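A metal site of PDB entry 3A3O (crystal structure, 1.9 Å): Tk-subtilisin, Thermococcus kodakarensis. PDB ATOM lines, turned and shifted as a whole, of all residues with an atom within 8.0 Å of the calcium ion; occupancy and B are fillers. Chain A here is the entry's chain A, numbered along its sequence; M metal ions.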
ATOM      1  N   GLN A  12     -10.738  34.044  15.355  1.00  0.00           N
ATOM      2  CA  GLN A  12     -11.560  32.872  14.864  1.00  0.00           C
ATOM      3  C   GLN A  12     -12.020  33.094  13.425  1.00  0.00           C
ATOM      4  O   GLN A  12     -12.612  34.128  13.127  1.00  0.00           O
ATOM      5  CB  GLN A  12     -12.781  32.630  15.761  1.00  0.00           C
ATOM      6  CG  GLN A  12     -12.474  32.001  17.124  1.00  0.00           C
ATOM      7  CD  GLN A  12     -11.957  30.565  17.014  1.00  0.00           C
ATOM      8  OE1 GLN A  12     -12.411  29.788  16.176  1.00  0.00           O
ATOM      9  NE2 GLN A  12     -10.977  30.217  17.837  1.00  0.00           N
ATOM     10  N   PRO A  13     -11.784  32.107  12.532  1.00  0.00           N
ATOM     11  CA  PRO A  13     -12.266  32.248  11.158  1.00  0.00           C
ATOM     12  C   PRO A  13     -13.779  32.112  11.034  1.00  0.00           C
ATOM     13  O   PRO A  13     -14.415  31.487  11.909  1.00  0.00           O
ATOM     14  CB  PRO A  13     -11.579  31.093  10.415  1.00  0.00           C
ATOM     15  CG  PRO A  13     -11.292  30.050  11.505  1.00  0.00           C
ATOM     16  CD  PRO A  13     -11.079  30.833  12.787  1.00  0.00           C
ATOM     17  N   ALA A  14     -14.351  32.681   9.955  1.00  0.00           N
ATOM     18  CA  ALA A  14     -15.767  32.517   9.602  1.00  0.00           C
ATOM     19  C   ALA A  14     -16.080  31.047   9.334  1.00  0.00           C
ATOM     20  O   ALA A  14     -15.216  30.310   8.816  1.00  0.00           O
ATOM     21  CB  ALA A  14     -16.120  33.368   8.384  1.00  0.00           C
ATOM     22  N   GLN A  15     -17.302  30.637   9.681  1.00  0.00           N
ATOM     23  CA  GLN A  15     -17.708  29.221   9.578  1.00  0.00           C
ATOM     24  C   GLN A  15     -17.730  28.700   8.142  1.00  0.00           C
ATOM     25  O   GLN A  15     -18.244  29.366   7.234  1.00  0.00           O
ATOM     26  CB  GLN A  15     -19.080  28.989  10.225  1.00  0.00           C
ATOM     27  CG  GLN A  15     -19.532  27.521  10.248  1.00  0.00           C
ATOM     28  CD  GLN A  15     -20.734  27.284  11.108  1.00  0.00           C
ATOM     29  OE1 GLN A  15     -20.614  27.205  12.332  1.00  0.00           O
ATOM     30  NE2 GLN A  15     -21.910  27.189  10.485  1.00  0.00           N
ATOM     31  N   THR A  16     -17.141  27.509   7.933  1.00  0.00           N
ATOM     32  CA  THR A  16     -17.400  26.735   6.713  1.00  0.00           C
ATOM     33  C   THR A  16     -18.028  25.427   7.075  1.00  0.00           C
ATOM     34  O   THR A  16     -17.840  24.942   8.191  1.00  0.00           O
ATOM     35  CB  THR A  16     -16.140  26.180   6.030  1.00  0.00           C
ATOM     36  OG1 THR A  16     -14.955  26.479   6.787  1.00  0.00           O
ATOM     37  CG2 THR A  16     -16.083  26.533   4.558  1.00  0.00           C
ATOM     38  N   HIS A  53     -12.607  25.153  23.672  1.00  0.00           N
ATOM     39  CA  HIS A  53     -12.639  25.588  22.280  1.00  0.00           C
ATOM     40  C   HIS A  53     -13.948  26.323  21.998  1.00  0.00           C
ATOM     41  O   HIS A  53     -15.026  25.827  22.328  1.00  0.00           O
ATOM     42  CB  HIS A  53     -12.461  24.396  21.334  1.00  0.00           C
ATOM     43  CG  HIS A  53     -12.231  24.797  19.910  1.00  0.00           C
ATOM     44  ND1 HIS A  53     -11.113  24.420  19.209  1.00  0.00           N
ATOM     45  CD2 HIS A  53     -12.970  25.551  19.069  1.00  0.00           C
ATOM     46  CE1 HIS A  53     -11.182  24.898  17.977  1.00  0.00           C
ATOM     47  NE2 HIS A  53     -12.291  25.608  17.870  1.00  0.00           N
ATOM     48  N   PRO A  54     -13.892  27.547  21.436  1.00  0.00           N
ATOM     49  CA  PRO A  54     -15.144  28.305  21.190  1.00  0.00           C
ATOM     50  C   PRO A  54     -16.132  27.592  20.266  1.00  0.00           C
ATOM     51  O   PRO A  54     -17.350  27.861  20.301  1.00  0.00           O
ATOM     52  CB  PRO A  54     -14.660  29.602  20.510  1.00  0.00           C
ATOM     53  CG  PRO A  54     -13.233  29.749  20.927  1.00  0.00           C
ATOM     54  CD  PRO A  54     -12.685  28.324  21.061  1.00  0.00           C
ATOM     55  N   ASP A  55     -15.637  26.686  19.428  1.00  0.00           N
ATOM     56  CA  ASP A  55     -16.545  25.954  18.523  1.00  0.00           C
ATOM     57  C   ASP A  55     -16.997  24.595  19.056  1.00  0.00           C
ATOM     58  O   ASP A  55     -17.660  23.837  18.330  1.00  0.00           O
ATOM     59  CB  ASP A  55     -15.968  25.812  17.104  1.00  0.00           C
ATOM     60  CG  ASP A  55     -17.040  26.032  16.036  1.00  0.00           C
ATOM     61  OD1 ASP A  55     -18.062  26.702  16.315  1.00  0.00           O
ATOM     62  OD2 ASP A  55     -16.895  25.568  14.890  1.00  0.00           O
ATOM     63  N   LEU A  56     -16.639  24.311  20.323  1.00  0.00           N
ATOM     64  CA  LEU A  56     -16.992  23.048  20.991  1.00  0.00           C
ATOM     65  C   LEU A  56     -17.636  23.203  22.358  1.00  0.00           C
ATOM     66  O   LEU A  56     -18.436  22.349  22.791  1.00  0.00           O
ATOM     67  CB  LEU A  56     -15.745  22.176  21.170  1.00  0.00           C
ATOM     68  CG  LEU A  56     -14.981  21.611  19.957  1.00  0.00           C
ATOM     69  CD1 LEU A  56     -13.917  20.688  20.492  1.00  0.00           C
ATOM     70  CD2 LEU A  56     -15.896  20.857  19.013  1.00  0.00           C
ATOM     71  N   ALA A  93     -19.741  17.315  16.468  1.00  0.00           N
ATOM     72  CA  ALA A  93     -20.525  18.261  17.297  1.00  0.00           C
ATOM     73  C   ALA A  93     -20.041  19.702  17.308  1.00  0.00           C
ATOM     74  O   ALA A  93     -20.462  20.488  18.194  1.00  0.00           O
ATOM     75  CB  ALA A  93     -20.595  17.742  18.713  1.00  0.00           C
ATOM     76  N   ALA A  94     -19.182  20.075  16.343  1.00  0.00           N
ATOM     77  CA  ALA A  94     -18.804  21.506  16.254  1.00  0.00           C
ATOM     78  C   ALA A  94     -20.084  22.352  16.092  1.00  0.00           C
ATOM     79  O   ALA A  94     -21.005  21.966  15.370  1.00  0.00           O
ATOM     80  CB  ALA A  94     -17.845  21.750  15.106  1.00  0.00           C
ATOM     81  N   LEU A  95     -20.146  23.496  16.773  1.00  0.00           N
ATOM     82  CA  LEU A  95     -21.380  24.283  16.847  1.00  0.00           C
ATOM     83  C   LEU A  95     -21.708  24.976  15.524  1.00  0.00           C
ATOM     84  O   LEU A  95     -20.799  25.404  14.783  1.00  0.00           O
ATOM     85  CB  LEU A  95     -21.222  25.318  17.973  1.00  0.00           C
ATOM     86  CG  LEU A  95     -21.137  24.718  19.380  1.00  0.00           C
ATOM     87  CD1 LEU A  95     -20.275  25.578  20.349  1.00  0.00           C
ATOM     88  CD2 LEU A  95     -22.536  24.512  19.955  1.00  0.00           C
ATOM     89  N   ASN A  96     -23.000  25.079  15.232  1.00  0.00           N
ATOM     90  CA  ASN A  96     -23.474  25.803  14.055  1.00  0.00           C
ATOM     91  C   ASN A  96     -23.645  27.272  14.462  1.00  0.00           C
ATOM     92  O   ASN A  96     -24.595  27.622  15.160  1.00  0.00           O
ATOM     93  CB  ASN A  96     -24.794  25.231  13.586  1.00  0.00           C
ATOM     94  CG  ASN A  96     -25.240  25.797  12.245  1.00  0.00           C
ATOM     95  OD1 ASN A  96     -24.525  26.597  11.640  1.00  0.00           O
ATOM     96  ND2 ASN A  96     -26.408  25.386  11.782  1.00  0.00           N
ATOM     97  N   ASN A  97     -22.696  28.109  14.056  1.00  0.00           N
ATOM     98  CA  ASN A  97     -22.632  29.498  14.520  1.00  0.00           C
ATOM     99  C   ASN A  97     -21.888  30.330  13.475  1.00  0.00           C
ATOM    100  O   ASN A  97     -21.879  29.976  12.301  1.00  0.00           O
ATOM    101  CB  ASN A  97     -21.964  29.564  15.931  1.00  0.00           C
ATOM    102  CG  ASN A  97     -20.573  28.887  15.986  1.00  0.00           C
ATOM    103  OD1 ASN A  97     -19.960  28.584  14.954  1.00  0.00           O
ATOM    104  ND2 ASN A  97     -20.054  28.687  17.206  1.00  0.00           N
ATOM    105  N   ASP A  98     -21.201  31.378  13.911  1.00  0.00           N
ATOM    106  CA  ASP A  98     -20.520  32.248  12.969  1.00  0.00           C
ATOM    107  C   ASP A  98     -19.059  31.916  12.723  1.00  0.00           C
ATOM    108  O   ASP A  98     -18.402  32.603  11.953  1.00  0.00           O
ATOM    109  CB  ASP A  98     -20.683  33.726  13.397  1.00  0.00           C
ATOM    110  CG  ASP A  98     -22.140  34.151  13.469  1.00  0.00           C
ATOM    111  OD1 ASP A  98     -22.906  33.875  12.502  1.00  0.00           O
ATOM    112  OD2 ASP A  98     -22.543  34.763  14.496  1.00  0.00           O
ATOM    113  N   ILE A  99     -18.555  30.864  13.364  1.00  0.00           N
ATOM    114  CA  ILE A  99     -17.124  30.562  13.355  1.00  0.00           C
ATOM    115  C   ILE A  99     -16.764  29.105  13.028  1.00  0.00           C
ATOM    116  O   ILE A  99     -17.559  28.199  13.250  1.00  0.00           O
ATOM    117  CB  ILE A  99     -16.452  30.920  14.717  1.00  0.00           C
ATOM    118  CG1 ILE A  99     -17.160  30.195  15.885  1.00  0.00           C
ATOM    119  CG2 ILE A  99     -16.471  32.468  14.953  1.00  0.00           C
ATOM    120  CD1 ILE A  99     -16.313  30.098  17.138  1.00  0.00           C
ATOM    121  N   GLY A 100     -15.566  28.897  12.508  1.00  0.00           N
ATOM    122  CA  GLY A 100     -14.934  27.590  12.532  1.00  0.00           C
ATOM    123  C   GLY A 100     -15.560  26.597  11.586  1.00  0.00           C
ATOM    124  O   GLY A 100     -15.565  26.811  10.370  1.00  0.00           O
ATOM    125  N   VAL A 101     -16.052  25.481  12.109  1.00  0.00           N
ATOM    126  CA  VAL A 101     -16.644  24.447  11.257  1.00  0.00           C
ATOM    127  C   VAL A 101     -18.035  24.120  11.811  1.00  0.00           C
ATOM    128  O   VAL A 101     -18.588  24.918  12.574  1.00  0.00           O
ATOM    129  CB  VAL A 101     -15.709  23.208  11.143  1.00  0.00           C
ATOM    130  CG1 VAL A 101     -14.442  23.543  10.331  1.00  0.00           C
ATOM    131  CG2 VAL A 101     -15.338  22.629  12.557  1.00  0.00           C
ATOM    132  N   VAL A 102     -18.625  22.985  11.440  1.00  0.00           N
ATOM    133  CA  VAL A 102     -19.909  22.568  12.000  1.00  0.00           C
ATOM    134  C   VAL A 102     -19.936  21.040  11.947  1.00  0.00           C
ATOM    135  O   VAL A 102     -19.477  20.465  10.975  1.00  0.00           O
ATOM    136  CB  VAL A 102     -21.123  23.204  11.251  1.00  0.00           C
ATOM    137  CG1 VAL A 102     -21.172  22.812   9.751  1.00  0.00           C
ATOM    138  CG2 VAL A 102     -22.441  22.920  11.961  1.00  0.00           C
ATOM    139  N   GLY A 103     -20.471  20.412  13.003  1.00  0.00           N
ATOM    140  CA  GLY A 103     -20.496  18.941  13.093  1.00  0.00           C
ATOM    141  C   GLY A 103     -21.708  18.387  12.372  1.00  0.00           C
ATOM    142  O   GLY A 103     -22.596  19.132  11.941  1.00  0.00           O
ATOM    143  N   PRO A 106     -24.682  19.254  15.251  1.00  0.00           N
ATOM    144  CA  PRO A 106     -24.095  20.403  15.895  1.00  0.00           C
ATOM    145  C   PRO A 106     -24.723  20.846  17.234  1.00  0.00           C
ATOM    146  O   PRO A 106     -24.182  21.763  17.846  1.00  0.00           O
ATOM    147  CB  PRO A 106     -24.182  21.496  14.820  1.00  0.00           C
ATOM    148  CG  PRO A 106     -25.245  21.123  13.919  1.00  0.00           C
ATOM    149  CD  PRO A 106     -25.360  19.601  13.990  1.00  0.00           C
ATOM    150  N   THR A 242     -12.023  20.920  14.275  1.00  0.00           N
ATOM    151  CA  THR A 242     -11.410  21.600  15.408  1.00  0.00           C
ATOM    152  C   THR A 242     -10.069  20.931  15.804  1.00  0.00           C
ATOM    153  O   THR A 242      -9.869  19.721  15.608  1.00  0.00           O
ATOM    154  CB  THR A 242     -12.396  21.645  16.601  1.00  0.00           C
ATOM    155  OG1 THR A 242     -12.990  20.346  16.758  1.00  0.00           O
ATOM    156  CG2 THR A 242     -13.550  22.658  16.290  1.00  0.00           C
ATOM    157  N   TYR A 248      -7.932  24.877  14.144  1.00  0.00           N
ATOM    158  CA  TYR A 248      -8.553  23.945  13.176  1.00  0.00           C
ATOM    159  C   TYR A 248      -7.417  23.238  12.458  1.00  0.00           C
ATOM    160  O   TYR A 248      -6.300  23.781  12.368  1.00  0.00           O
ATOM    161  CB  TYR A 248      -9.529  24.685  12.197  1.00  0.00           C
ATOM    162  CG  TYR A 248     -10.560  25.446  12.959  1.00  0.00           C
ATOM    163  CD1 TYR A 248     -10.278  26.744  13.426  1.00  0.00           C
ATOM    164  CD2 TYR A 248     -11.757  24.845  13.354  1.00  0.00           C
ATOM    165  CE1 TYR A 248     -11.157  27.426  14.216  1.00  0.00           C
ATOM    166  CE2 TYR A 248     -12.659  25.524  14.140  1.00  0.00           C
ATOM    167  CZ  TYR A 248     -12.351  26.823  14.574  1.00  0.00           C
ATOM    168  OH  TYR A 248     -13.235  27.502  15.372  1.00  0.00           O
HETATM  169 CA    CA M   1     -19.030  26.616  14.054  1.00  0.00          CA
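The calcium ion is bound by O of Leu 95 (2.3 Å), O of Val 101 (2.3 Å), O of Ile 99 (2.3 Å), OD1 of Asn 97 (2.4 Å), OE1 of Gln 15 (2.4 Å), OD1 of Asp 55 (2.5 Å) and OD2 of Asp 55 (2.5 Å).
The calcium ion has seven donor atoms within binding distance.
The side-chain amide nitrogen (NE2) of Gln 15 sits at hydrogen-bond distance from the side-chain amide oxygen (OD1) of Asn 96.
The backbone NH (N) of Gln 15 lies within hydrogen-bond range of the backbone carbonyl oxygen (O) of Asp 98 (3.2 Å).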
